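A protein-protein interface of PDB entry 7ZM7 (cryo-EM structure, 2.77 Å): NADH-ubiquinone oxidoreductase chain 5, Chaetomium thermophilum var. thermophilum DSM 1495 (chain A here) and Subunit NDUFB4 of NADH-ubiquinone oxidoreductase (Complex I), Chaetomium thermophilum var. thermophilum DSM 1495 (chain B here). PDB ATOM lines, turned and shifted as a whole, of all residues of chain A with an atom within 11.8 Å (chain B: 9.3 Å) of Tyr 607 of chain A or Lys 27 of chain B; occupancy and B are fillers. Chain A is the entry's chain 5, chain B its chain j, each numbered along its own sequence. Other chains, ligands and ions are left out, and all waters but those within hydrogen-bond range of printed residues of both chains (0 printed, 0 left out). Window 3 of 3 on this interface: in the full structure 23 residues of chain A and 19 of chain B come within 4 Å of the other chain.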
ATOM      1  N   THR A 593      15.353 -23.426   3.548  1.00  0.00           N
ATOM      2  CA  THR A 593      16.645 -22.819   3.851  1.00  0.00           C
ATOM      3  C   THR A 593      17.765 -23.849   3.838  1.00  0.00           C
ATOM      4  O   THR A 593      18.828 -23.614   3.254  1.00  0.00           O
ATOM      5  CB  THR A 593      16.598 -22.110   5.206  1.00  0.00           C
ATOM      6  OG1 THR A 593      15.509 -21.186   5.240  1.00  0.00           O
ATOM      7  CG2 THR A 593      17.891 -21.358   5.456  1.00  0.00           C
ATOM      8  N   LYS A 594      17.559 -24.990   4.490  1.00  0.00           N
ATOM      9  CA  LYS A 594      18.657 -25.937   4.646  1.00  0.00           C
ATOM     10  C   LYS A 594      18.812 -26.843   3.435  1.00  0.00           C
ATOM     11  O   LYS A 594      19.910 -26.987   2.898  1.00  0.00           O
ATOM     12  CB  LYS A 594      18.468 -26.783   5.901  1.00  0.00           C
ATOM     13  CG  LYS A 594      18.505 -26.015   7.184  1.00  0.00           C
ATOM     14  CD  LYS A 594      18.387 -26.980   8.363  1.00  0.00           C
ATOM     15  CE  LYS A 594      17.012 -27.614   8.527  1.00  0.00           C
ATOM     16  NZ  LYS A 594      15.978 -26.623   8.893  1.00  0.00           N
ATOM     17  N   ILE A 595      17.731 -27.486   3.010  1.00  0.00           N
ATOM     18  CA  ILE A 595      17.861 -28.511   1.988  1.00  0.00           C
ATOM     19  C   ILE A 595      18.029 -27.906   0.605  1.00  0.00           C
ATOM     20  O   ILE A 595      18.700 -28.494  -0.248  1.00  0.00           O
ATOM     21  CB  ILE A 595      16.660 -29.469   2.051  1.00  0.00           C
ATOM     22  CG1 ILE A 595      16.578 -30.097   3.443  1.00  0.00           C
ATOM     23  CG2 ILE A 595      16.757 -30.533   0.965  1.00  0.00           C
ATOM     24  CD1 ILE A 595      15.539 -31.126   3.577  1.00  0.00           C
ATOM     25  N   LEU A 596      17.475 -26.722   0.353  1.00  0.00           N
ATOM     26  CA  LEU A 596      17.487 -26.178  -0.995  1.00  0.00           C
ATOM     27  C   LEU A 596      18.444 -25.008  -1.145  1.00  0.00           C
ATOM     28  O   LEU A 596      19.397 -25.106  -1.920  1.00  0.00           O
ATOM     29  CB  LEU A 596      16.078 -25.753  -1.424  1.00  0.00           C
ATOM     30  CG  LEU A 596      14.900 -26.644  -1.040  1.00  0.00           C
ATOM     31  CD1 LEU A 596      13.639 -26.060  -1.566  1.00  0.00           C
ATOM     32  CD2 LEU A 596      15.069 -28.032  -1.560  1.00  0.00           C
ATOM     33  N   ASP A 597      18.239 -23.918  -0.406  1.00  0.00           N
ATOM     34  CA  ASP A 597      19.058 -22.721  -0.595  1.00  0.00           C
ATOM     35  C   ASP A 597      20.520 -23.018  -0.357  1.00  0.00           C
ATOM     36  O   ASP A 597      21.392 -22.565  -1.101  1.00  0.00           O
ATOM     37  CB  ASP A 597      18.623 -21.612   0.356  1.00  0.00           C
ATOM     38  CG  ASP A 597      17.282 -21.053   0.018  1.00  0.00           C
ATOM     39  OD1 ASP A 597      16.921 -21.071  -1.169  1.00  0.00           O
ATOM     40  OD2 ASP A 597      16.582 -20.599   0.929  1.00  0.00           O
ATOM     41  N   LYS A 598      20.804 -23.744   0.716  1.00  0.00           N
ATOM     42  CA  LYS A 598      22.153 -24.046   1.149  1.00  0.00           C
ATOM     43  C   LYS A 598      22.525 -25.465   0.766  1.00  0.00           C
ATOM     44  O   LYS A 598      23.411 -26.074   1.364  1.00  0.00           O
ATOM     45  CB  LYS A 598      22.243 -23.829   2.653  1.00  0.00           C
ATOM     46  CG  LYS A 598      21.896 -22.410   3.005  1.00  0.00           C
ATOM     47  CD  LYS A 598      22.909 -21.451   2.440  1.00  0.00           C
ATOM     48  CE  LYS A 598      22.669 -20.032   2.911  1.00  0.00           C
ATOM     49  NZ  LYS A 598      21.425 -19.489   2.309  1.00  0.00           N
ATOM     50  N   GLY A 599      21.820 -26.006  -0.211  1.00  0.00           N
ATOM     51  CA  GLY A 599      21.861 -27.402  -0.551  1.00  0.00           C
ATOM     52  C   GLY A 599      21.877 -27.636  -2.040  1.00  0.00           C
ATOM     53  O   GLY A 599      22.821 -27.282  -2.740  1.00  0.00           O
ATOM     54  N   SER A 600      20.818 -28.286  -2.509  1.00  0.00           N
ATOM     55  CA  SER A 600      20.673 -28.636  -3.912  1.00  0.00           C
ATOM     56  C   SER A 600      20.761 -27.433  -4.844  1.00  0.00           C
ATOM     57  O   SER A 600      21.155 -27.570  -6.002  1.00  0.00           O
ATOM     58  CB  SER A 600      19.350 -29.360  -4.090  1.00  0.00           C
ATOM     59  OG  SER A 600      18.276 -28.491  -3.809  1.00  0.00           O
ATOM     60  N   ILE A 601      20.367 -26.249  -4.385  1.00  0.00           N
ATOM     61  CA  ILE A 601      20.533 -25.079  -5.239  1.00  0.00           C
ATOM     62  C   ILE A 601      22.010 -24.750  -5.403  1.00  0.00           C
ATOM     63  O   ILE A 601      22.455 -24.340  -6.480  1.00  0.00           O
ATOM     64  CB  ILE A 601      19.722 -23.890  -4.700  1.00  0.00           C
ATOM     65  CG1 ILE A 601      18.236 -24.238  -4.686  1.00  0.00           C
ATOM     66  CG2 ILE A 601      19.986 -22.642  -5.509  1.00  0.00           C
ATOM     67  CD1 ILE A 601      17.678 -24.628  -6.002  1.00  0.00           C
ATOM     68  N   GLU A 602      22.797 -24.935  -4.351  1.00  0.00           N
ATOM     69  CA  GLU A 602      24.222 -24.680  -4.484  1.00  0.00           C
ATOM     70  C   GLU A 602      24.982 -25.905  -4.984  1.00  0.00           C
ATOM     71  O   GLU A 602      25.969 -25.763  -5.707  1.00  0.00           O
ATOM     72  CB  GLU A 602      24.768 -24.145  -3.166  1.00  0.00           C
ATOM     73  CG  GLU A 602      24.197 -22.776  -2.895  1.00  0.00           C
ATOM     74  CD  GLU A 602      24.659 -22.164  -1.615  1.00  0.00           C
ATOM     75  OE1 GLU A 602      25.331 -22.862  -0.869  1.00  0.00           O
ATOM     76  OE2 GLU A 602      24.368 -20.978  -1.353  1.00  0.00           O
ATOM     77  N   LEU A 603      24.534 -27.116  -4.643  1.00  0.00           N
ATOM     78  CA  LEU A 603      25.169 -28.299  -5.223  1.00  0.00           C
ATOM     79  C   LEU A 603      24.865 -28.427  -6.704  1.00  0.00           C
ATOM     80  O   LEU A 603      25.757 -28.755  -7.490  1.00  0.00           O
ATOM     81  CB  LEU A 603      24.745 -29.578  -4.508  1.00  0.00           C
ATOM     82  CG  LEU A 603      25.607 -30.802  -4.859  1.00  0.00           C
ATOM     83  CD1 LEU A 603      27.082 -30.473  -4.723  1.00  0.00           C
ATOM     84  CD2 LEU A 603      25.271 -32.020  -4.019  1.00  0.00           C
ATOM     85  N   PHE A 604      23.626 -28.172  -7.106  1.00  0.00           N
ATOM     86  CA  PHE A 604      23.264 -28.070  -8.518  1.00  0.00           C
ATOM     87  C   PHE A 604      23.407 -26.640  -9.014  1.00  0.00           C
ATOM     88  O   PHE A 604      22.424 -26.011  -9.405  1.00  0.00           O
ATOM     89  CB  PHE A 604      21.848 -28.590  -8.738  1.00  0.00           C
ATOM     90  CG  PHE A 604      21.492 -28.827 -10.164  1.00  0.00           C
ATOM     91  CD1 PHE A 604      22.456 -29.107 -11.094  1.00  0.00           C
ATOM     92  CD2 PHE A 604      20.180 -28.783 -10.568  1.00  0.00           C
ATOM     93  CE1 PHE A 604      22.129 -29.326 -12.408  1.00  0.00           C
ATOM     94  CE2 PHE A 604      19.844 -29.008 -11.885  1.00  0.00           C
ATOM     95  CZ  PHE A 604      20.827 -29.282 -12.805  1.00  0.00           C
ATOM     96  N   GLY A 605      24.618 -26.097  -8.955  1.00  0.00           N
ATOM     97  CA  GLY A 605      24.873 -24.739  -9.361  1.00  0.00           C
ATOM     98  C   GLY A 605      26.292 -24.311  -9.082  1.00  0.00           C
ATOM     99  O   GLY A 605      27.244 -25.018  -9.395  1.00  0.00           O
ATOM    100  N   PRO A 606      26.454 -23.141  -8.461  1.00  0.00           N
ATOM    101  CA  PRO A 606      27.805 -22.581  -8.286  1.00  0.00           C
ATOM    102  C   PRO A 606      28.772 -23.479  -7.535  1.00  0.00           C
ATOM    103  O   PRO A 606      29.941 -23.573  -7.913  1.00  0.00           O
ATOM    104  CB  PRO A 606      27.537 -21.286  -7.509  1.00  0.00           C
ATOM    105  CG  PRO A 606      26.109 -21.004  -7.705  1.00  0.00           C
ATOM    106  CD  PRO A 606      25.433 -22.308  -7.816  1.00  0.00           C
ATOM    107  N   TYR A 607      28.331 -24.138  -6.475  1.00  0.00           N
ATOM    108  CA  TYR A 607      29.251 -24.988  -5.733  1.00  0.00           C
ATOM    109  C   TYR A 607      29.484 -26.321  -6.431  1.00  0.00           C
ATOM    110  O   TYR A 607      30.577 -26.881  -6.352  1.00  0.00           O
ATOM    111  CB  TYR A 607      28.741 -25.197  -4.316  1.00  0.00           C
ATOM    112  CG  TYR A 607      29.793 -25.697  -3.385  1.00  0.00           C
ATOM    113  CD1 TYR A 607      31.014 -25.065  -3.289  1.00  0.00           C
ATOM    114  CD2 TYR A 607      29.559 -26.796  -2.586  1.00  0.00           C
ATOM    115  CE1 TYR A 607      31.973 -25.522  -2.431  1.00  0.00           C
ATOM    116  CE2 TYR A 607      30.503 -27.255  -1.736  1.00  0.00           C
ATOM    117  CZ  TYR A 607      31.702 -26.620  -1.653  1.00  0.00           C
ATOM    118  OH  TYR A 607      32.651 -27.092  -0.781  1.00  0.00           O
ATOM    119  N   GLY A 608      28.477 -26.843  -7.115  1.00  0.00           N
ATOM    120  CA  GLY A 608      28.698 -28.024  -7.924  1.00  0.00           C
ATOM    121  C   GLY A 608      29.605 -27.759  -9.105  1.00  0.00           C
ATOM    122  O   GLY A 608      30.498 -28.555  -9.400  1.00  0.00           O
ATOM    123  N   LEU A 609      29.386 -26.641  -9.796  1.00  0.00           N
ATOM    124  CA  LEU A 609      30.222 -26.291 -10.938  1.00  0.00           C
ATOM    125  C   LEU A 609      31.646 -25.992 -10.516  1.00  0.00           C
ATOM    126  O   LEU A 609      32.592 -26.366 -11.211  1.00  0.00           O
ATOM    127  CB  LEU A 609      29.640 -25.099 -11.673  1.00  0.00           C
ATOM    128  CG  LEU A 609      28.515 -25.408 -12.638  1.00  0.00           C
ATOM    129  CD1 LEU A 609      27.742 -24.139 -12.845  1.00  0.00           C
ATOM    130  CD2 LEU A 609      29.092 -25.908 -13.926  1.00  0.00           C
ATOM    131  N   GLU A 610      31.818 -25.309  -9.386  1.00  0.00           N
ATOM    132  CA  GLU A 610      33.152 -25.073  -8.847  1.00  0.00           C
ATOM    133  C   GLU A 610      33.888 -26.378  -8.595  1.00  0.00           C
ATOM    134  O   GLU A 610      35.031 -26.553  -9.023  1.00  0.00           O
ATOM    135  CB  GLU A 610      33.050 -24.285  -7.551  1.00  0.00           C
ATOM    136  CG  GLU A 610      34.378 -23.932  -6.964  1.00  0.00           C
ATOM    137  CD  GLU A 610      34.246 -23.122  -5.712  1.00  0.00           C
ATOM    138  OE1 GLU A 610      33.105 -22.861  -5.306  1.00  0.00           O
ATOM    139  OE2 GLU A 610      35.273 -22.745  -5.128  1.00  0.00           O
ATOM    140  N   ARG A 611      33.241 -27.314  -7.902  1.00  0.00           N
ATOM    141  CA  ARG A 611      33.913 -28.549  -7.532  1.00  0.00           C
ATOM    142  C   ARG A 611      34.246 -29.382  -8.758  1.00  0.00           C
ATOM    143  O   ARG A 611      35.339 -29.948  -8.849  1.00  0.00           O
ATOM    144  CB  ARG A 611      33.050 -29.350  -6.565  1.00  0.00           C
ATOM    145  CG  ARG A 611      33.198 -28.924  -5.153  1.00  0.00           C
ATOM    146  CD  ARG A 611      31.949 -29.213  -4.399  1.00  0.00           C
ATOM    147  NE  ARG A 611      31.446 -30.535  -4.735  1.00  0.00           N
ATOM    148  CZ  ARG A 611      31.554 -31.597  -3.944  1.00  0.00           C
ATOM    149  NH1 ARG A 611      31.058 -32.759  -4.330  1.00  0.00           N
ATOM    150  NH2 ARG A 611      32.177 -31.503  -2.781  1.00  0.00           N
ATOM    151  N   GLY A 612      33.321 -29.460  -9.709  1.00  0.00           N
ATOM    152  CA  GLY A 612      33.570 -30.244 -10.905  1.00  0.00           C
ATOM    153  C   GLY A 612      34.643 -29.654 -11.798  1.00  0.00           C
ATOM    154  O   GLY A 612      35.544 -30.363 -12.249  1.00  0.00           O
ATOM    155  N   LEU A 613      34.568 -28.353 -12.063  1.00  0.00           N
ATOM    156  CA  LEU A 613      35.471 -27.750 -13.031  1.00  0.00           C
ATOM    157  C   LEU A 613      36.912 -27.761 -12.537  1.00  0.00           C
ATOM    158  O   LEU A 613      37.835 -28.016 -13.315  1.00  0.00           O
ATOM    159  CB  LEU A 613      35.003 -26.332 -13.355  1.00  0.00           C
ATOM    160  CG  LEU A 613      33.790 -26.235 -14.281  1.00  0.00           C
ATOM    161  CD1 LEU A 613      33.451 -24.817 -14.544  1.00  0.00           C
ATOM    162  CD2 LEU A 613      34.017 -26.974 -15.580  1.00  0.00           C
ATOM    163  N   VAL A 614      37.127 -27.492 -11.250  1.00  0.00           N
ATOM    164  CA  VAL A 614      38.481 -27.485 -10.704  1.00  0.00           C
ATOM    165  C   VAL A 614      39.109 -28.863 -10.820  1.00  0.00           C
ATOM    166  O   VAL A 614      40.303 -28.998 -11.108  1.00  0.00           O
ATOM    167  CB  VAL A 614      38.463 -26.995  -9.248  1.00  0.00           C
ATOM    168  CG1 VAL A 614      39.740 -27.380  -8.540  1.00  0.00           C
ATOM    169  CG2 VAL A 614      38.259 -25.512  -9.204  1.00  0.00           C
ATOM    170  N   LYS A 615      38.327 -29.906 -10.562  1.00  0.00           N
ATOM    171  CA  LYS A 615      38.821 -31.255 -10.760  1.00  0.00           C
ATOM    172  C   LYS A 615      39.072 -31.533 -12.236  1.00  0.00           C
ATOM    173  O   LYS A 615      40.089 -32.134 -12.595  1.00  0.00           O
ATOM    174  CB  LYS A 615      37.833 -32.254 -10.171  1.00  0.00           C
ATOM    175  CG  LYS A 615      38.350 -33.667 -10.103  1.00  0.00           C
ATOM    176  CD  LYS A 615      37.337 -34.606  -9.461  1.00  0.00           C
ATOM    177  CE  LYS A 615      37.188 -34.348  -7.971  1.00  0.00           C
ATOM    178  NZ  LYS A 615      38.486 -34.456  -7.256  1.00  0.00           N
ATOM    179  N   LEU A 616      38.162 -31.094 -13.102  1.00  0.00           N
ATOM    180  CA  LEU A 616      38.345 -31.262 -14.536  1.00  0.00           C
ATOM    181  C   LEU A 616      39.665 -30.666 -14.997  1.00  0.00           C
ATOM    182  O   LEU A 616      40.440 -31.324 -15.693  1.00  0.00           O
ATOM    183  CB  LEU A 616      37.184 -30.603 -15.272  1.00  0.00           C
ATOM    184  CG  LEU A 616      37.118 -30.602 -16.798  1.00  0.00           C
ATOM    185  CD1 LEU A 616      36.949 -31.971 -17.322  1.00  0.00           C
ATOM    186  CD2 LEU A 616      36.029 -29.699 -17.309  1.00  0.00           C
ATOM    187  N   MET A 667      36.761 -35.417 -15.606  1.00  0.00           N
ATOM    188  CA  MET A 667      36.140 -35.203 -14.307  1.00  0.00           C
ATOM    189  C   MET A 667      36.471 -36.334 -13.349  1.00  0.00           C
ATOM    190  O   MET A 667      36.620 -36.103 -12.144  1.00  0.00           O
ATOM    191  CB  MET A 667      34.624 -35.074 -14.444  1.00  0.00           C
ATOM    192  CG  MET A 667      34.139 -33.809 -15.114  1.00  0.00           C
ATOM    193  SD  MET A 667      33.930 -32.453 -13.950  1.00  0.00           S
ATOM    194  CE  MET A 667      32.668 -31.474 -14.765  1.00  0.00           C
ATOM    195  N   SER B  20      28.935 -19.966  12.470  1.00  0.00           N
ATOM    196  CA  SER B  20      29.963 -20.518  11.605  1.00  0.00           C
ATOM    197  C   SER B  20      29.533 -21.852  11.022  1.00  0.00           C
ATOM    198  O   SER B  20      30.041 -22.263   9.972  1.00  0.00           O
ATOM    199  CB  SER B  20      31.261 -20.656  12.381  1.00  0.00           C
ATOM    200  OG  SER B  20      31.528 -19.453  13.070  1.00  0.00           O
ATOM    201  N   MET B  21      28.610 -22.546  11.681  1.00  0.00           N
ATOM    202  CA  MET B  21      28.064 -23.754  11.084  1.00  0.00           C
ATOM    203  C   MET B  21      27.173 -23.422   9.897  1.00  0.00           C
ATOM    204  O   MET B  21      27.249 -24.078   8.856  1.00  0.00           O
ATOM    205  CB  MET B  21      27.288 -24.552  12.121  1.00  0.00           C
ATOM    206  CG  MET B  21      26.887 -25.922  11.637  1.00  0.00           C
ATOM    207  SD  MET B  21      25.255 -25.946  10.883  1.00  0.00           S
ATOM    208  CE  MET B  21      24.234 -26.039  12.338  1.00  0.00           C
ATOM    209  N   ILE B  22      26.322 -22.410  10.047  1.00  0.00           N
ATOM    210  CA  ILE B  22      25.329 -22.087   9.032  1.00  0.00           C
ATOM    211  C   ILE B  22      25.993 -21.510   7.789  1.00  0.00           C
ATOM    212  O   ILE B  22      25.661 -21.880   6.659  1.00  0.00           O
ATOM    213  CB  ILE B  22      24.290 -21.124   9.628  1.00  0.00           C
ATOM    214  CG1 ILE B  22      23.254 -21.905  10.412  1.00  0.00           C
ATOM    215  CG2 ILE B  22      23.597 -20.366   8.546  1.00  0.00           C
ATOM    216  CD1 ILE B  22      22.414 -21.063  11.326  1.00  0.00           C
ATOM    217  N   SER B  23      26.957 -20.613   7.979  1.00  0.00           N
ATOM    218  CA  SER B  23      27.615 -19.974   6.849  1.00  0.00           C
ATOM    219  C   SER B  23      28.380 -20.972   5.999  1.00  0.00           C
ATOM    220  O   SER B  23      28.549 -20.757   4.794  1.00  0.00           O
ATOM    221  CB  SER B  23      28.554 -18.882   7.345  1.00  0.00           C
ATOM    222  OG  SER B  23      27.819 -17.822   7.926  1.00  0.00           O
ATOM    223  N   ASN B  24      28.859 -22.053   6.602  1.00  0.00           N
ATOM    224  CA  ASN B  24      29.623 -23.070   5.911  1.00  0.00           C
ATOM    225  C   ASN B  24      28.809 -24.314   5.620  1.00  0.00           C
ATOM    226  O   ASN B  24      29.372 -25.319   5.196  1.00  0.00           O
ATOM    227  CB  ASN B  24      30.851 -23.432   6.734  1.00  0.00           C
ATOM    228  CG  ASN B  24      31.891 -22.355   6.720  1.00  0.00           C
ATOM    229  OD1 ASN B  24      32.669 -22.250   5.780  1.00  0.00           O
ATOM    230  ND2 ASN B  24      31.926 -21.548   7.765  1.00  0.00           N
ATOM    231  N   ARG B  25      27.494 -24.261   5.813  1.00  0.00           N
ATOM    232  CA  ARG B  25      26.660 -25.460   5.779  1.00  0.00           C
ATOM    233  C   ARG B  25      26.689 -26.149   4.419  1.00  0.00           C
ATOM    234  O   ARG B  25      26.774 -27.375   4.347  1.00  0.00           O
ATOM    235  CB  ARG B  25      25.229 -25.088   6.146  1.00  0.00           C
ATOM    236  CG  ARG B  25      24.300 -26.252   6.216  1.00  0.00           C
ATOM    237  CD  ARG B  25      22.926 -25.845   6.659  1.00  0.00           C
ATOM    238  NE  ARG B  25      22.030 -26.992   6.624  1.00  0.00           N
ATOM    239  CZ  ARG B  25      21.867 -27.857   7.612  1.00  0.00           C
ATOM    240  NH1 ARG B  25      22.504 -27.698   8.753  1.00  0.00           N
ATOM    241  NH2 ARG B  25      21.037 -28.870   7.467  1.00  0.00           N
ATOM    242  N   TYR B  26      26.615 -25.378   3.340  1.00  0.00           N
ATOM    243  CA  TYR B  26      26.467 -25.924   1.997  1.00  0.00           C
ATOM    244  C   TYR B  26      27.639 -26.793   1.556  1.00  0.00           C
ATOM    245  O   TYR B  26      27.492 -27.573   0.614  1.00  0.00           O
ATOM    246  CB  TYR B  26      26.279 -24.771   1.012  1.00  0.00           C
ATOM    247  CG  TYR B  26      27.548 -23.996   0.808  1.00  0.00           C
ATOM    248  CD1 TYR B  26      27.954 -23.064   1.742  1.00  0.00           C
ATOM    249  CD2 TYR B  26      28.370 -24.236  -0.278  1.00  0.00           C
ATOM    250  CE1 TYR B  26      29.108 -22.381   1.596  1.00  0.00           C
ATOM    251  CE2 TYR B  26      29.537 -23.555  -0.432  1.00  0.00           C
ATOM    252  CZ  TYR B  26      29.909 -22.631   0.513  1.00  0.00           C
ATOM    253  OH  TYR B  26      31.078 -21.933   0.379  1.00  0.00           O
ATOM    254  N   LYS B  27      28.800 -26.666   2.186  1.00  0.00           N
ATOM    255  CA  LYS B  27      29.940 -27.474   1.795  1.00  0.00           C
ATOM    256  C   LYS B  27      29.715 -28.948   2.071  1.00  0.00           C
ATOM    257  O   LYS B  27      30.451 -29.788   1.548  1.00  0.00           O
ATOM    258  CB  LYS B  27      31.179 -27.013   2.536  1.00  0.00           C
ATOM    259  CG  LYS B  27      31.644 -25.647   2.170  1.00  0.00           C
ATOM    260  CD  LYS B  27      32.950 -25.351   2.822  1.00  0.00           C
ATOM    261  CE  LYS B  27      32.775 -25.097   4.282  1.00  0.00           C
ATOM    262  NZ  LYS B  27      34.057 -24.691   4.911  1.00  0.00           N
ATOM    263  N   TYR B  28      28.705 -29.281   2.870  1.00  0.00           N
ATOM    264  CA  TYR B  28      28.489 -30.644   3.308  1.00  0.00           C
ATOM    265  C   TYR B  28      27.190 -31.240   2.797  1.00  0.00           C
ATOM    266  O   TYR B  28      26.847 -32.352   3.186  1.00  0.00           O
ATOM    267  CB  TYR B  28      28.541 -30.734   4.830  1.00  0.00           C
ATOM    268  CG  TYR B  28      29.696 -30.016   5.453  1.00  0.00           C
ATOM    269  CD1 TYR B  28      29.699 -28.642   5.591  1.00  0.00           C
ATOM    270  CD2 TYR B  28      30.824 -30.704   5.828  1.00  0.00           C
ATOM    271  CE1 TYR B  28      30.749 -28.000   6.138  1.00  0.00           C
ATOM    272  CE2 TYR B  28      31.884 -30.065   6.370  1.00  0.00           C
ATOM    273  CZ  TYR B  28      31.847 -28.718   6.524  1.00  0.00           C
ATOM    274  OH  TYR B  28      32.928 -28.075   7.073  1.00  0.00           O
ATOM    275  N   PHE B  29      26.476 -30.552   1.921  1.00  0.00           N
ATOM    276  CA  PHE B  29      25.262 -31.118   1.362  1.00  0.00           C
ATOM    277  C   PHE B  29      25.591 -32.282   0.437  1.00  0.00           C
ATOM    278  O   PHE B  29      26.501 -32.205  -0.391  1.00  0.00           O
ATOM    279  CB  PHE B  29      24.473 -30.053   0.607  1.00  0.00           C
ATOM    280  CG  PHE B  29      23.242 -30.580  -0.054  1.00  0.00           C
ATOM    281  CD1 PHE B  29      22.064 -30.679   0.638  1.00  0.00           C
ATOM    282  CD2 PHE B  29      23.277 -31.010  -1.360  1.00  0.00           C
ATOM    283  CE1 PHE B  29      20.954 -31.176   0.040  1.00  0.00           C
ATOM    284  CE2 PHE B  29      22.163 -31.513  -1.959  1.00  0.00           C
ATOM    285  CZ  PHE B  29      20.999 -31.590  -1.257  1.00  0.00           C
ATOM    286  N   ARG B  30      24.844 -33.372   0.624  1.00  0.00           N
ATOM    287  CA  ARG B  30      25.060 -34.567  -0.220  1.00  0.00           C
ATOM    288  C   ARG B  30      23.770 -34.959  -0.939  1.00  0.00           C
ATOM    289  O   ARG B  30      22.698 -34.534  -0.501  1.00  0.00           O
ATOM    290  CB  ARG B  30      25.500 -35.749   0.644  1.00  0.00           C
ATOM    291  CG  ARG B  30      26.959 -35.779   1.065  1.00  0.00           C
ATOM    292  CD  ARG B  30      27.102 -37.079   1.835  1.00  0.00           C
ATOM    293  NE  ARG B  30      25.904 -37.301   2.634  1.00  0.00           N
ATOM    294  CZ  ARG B  30      25.858 -37.288   3.961  1.00  0.00           C
ATOM    295  NH1 ARG B  30      26.961 -37.095   4.661  1.00  0.00           N
ATOM    296  NH2 ARG B  30      24.712 -37.478   4.585  1.00  0.00           N
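The side-chain amino group (NZ) of Lys 27 of chain B is in hydrogen-bond range of the side-chain amide oxygen (OD1) of Asn 24 of chain B, 2.9 Å away. O of Thr 593 of chain A lies within hydrogen-bond range of N of Lys 598 of chain A (3.2 Å). O of Ile 595 of chain A lies within hydrogen-bond range of N of Ser 600 of chain A, at 3.1 Å. The backbone NH (N) of Tyr 607 of chain A sits at hydrogen-bond distance from the backbone carbonyl oxygen (O) of Glu 602 of chain A. The backbone NH of Gly 608 of chain A lies within hydrogen-bond range of the backbone carbonyl oxygen of Glu 602 of chain A (3.1 Å). O of Leu 603 of chain A lies close to N of Gly 608 of chain A, at 3.3 Å.
Among the printed residues, merely in contact across the chains: Lys 594 of chain A with Arg 25 of chain B, Ile 595 of chain A with Phe 29 of chain B, Lys 598 of chain A with Tyr 26 of chain B, Gly 599 of chain A with Phe 29 of chain B, Ser 600 of chain A with Phe 29 of chain B, Glu 602 of chain A with Tyr 26 of chain B, Leu 603 of chain A with Phe 29 of chain B, Tyr 607 of chain A with Tyr 26 of chain B and Tyr 607 of chain A with Lys 27 of chain B.
Of the printed residues of chain B, Lys 598 of chain A touches Tyr 26 (3.1 Å). Printed residues of chain B within 4 Å of Leu 603 of chain A: Phe 29. No residue of chain B comes within 4 Å of Gly 605 of chain A. No residue of chain B comes within 4 Å of Pro 606 of chain A. Tyr 607 of chain A touches just these residues of chain B: Tyr 26 and Lys 27. No residue of chain B comes within 4 Å of Gly 608 of chain A. No residue of chain B comes within 4 Å of Glu 610 of chain A. Met 667 of chain A touches none of the printed residues of chain B. No residue of chain A comes within 4 Å of Asn 24 of chain B. Of the printed residues of chain A, Arg 25 of chain B touches Lys 594 (3.4 Å). Of chain A, only Lys 598 (3.1 Å), Glu 602 (2.8 Å) and Tyr 607 (3.6 Å) come within 4 Å of Tyr 26 of chain B. Lys 27 of chain B touches just one residue of chain A: Tyr 607. Tyr 28 of chain B touches none of the printed residues of chain A. The nearest residue of chain B that does not touch Tyr 607 of chain A is Tyr 28 of chain B (5.3 Å). The nearest residue of chain A that does not touch Lys 27 of chain B is Arg 611 of chain A (5.0 Å). The nearest printed residue of chain B that does not touch Lys 594 of chain A is Phe 29 of chain B (4.8 Å).
Hydrophobic or aromatic side chains of chain B within 4 Å of the printed part of chain A: Tyr 26 and Phe 29. Of the 25 printed residues of chain A, 8 touch a printed residue of chain B. Printed residues of chain A that touch a printed residue of chain B: Lys 594, Ile 595, Lys 598, Gly 599, Ser 600, Glu 602, Leu 603 and Tyr 607. Hydrophobic or aromatic side chains of chain A within 4 Å of the printed part of chain B: Leu 603 and Tyr 607. Among the printed residues, 9 pairs touch across the chains.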
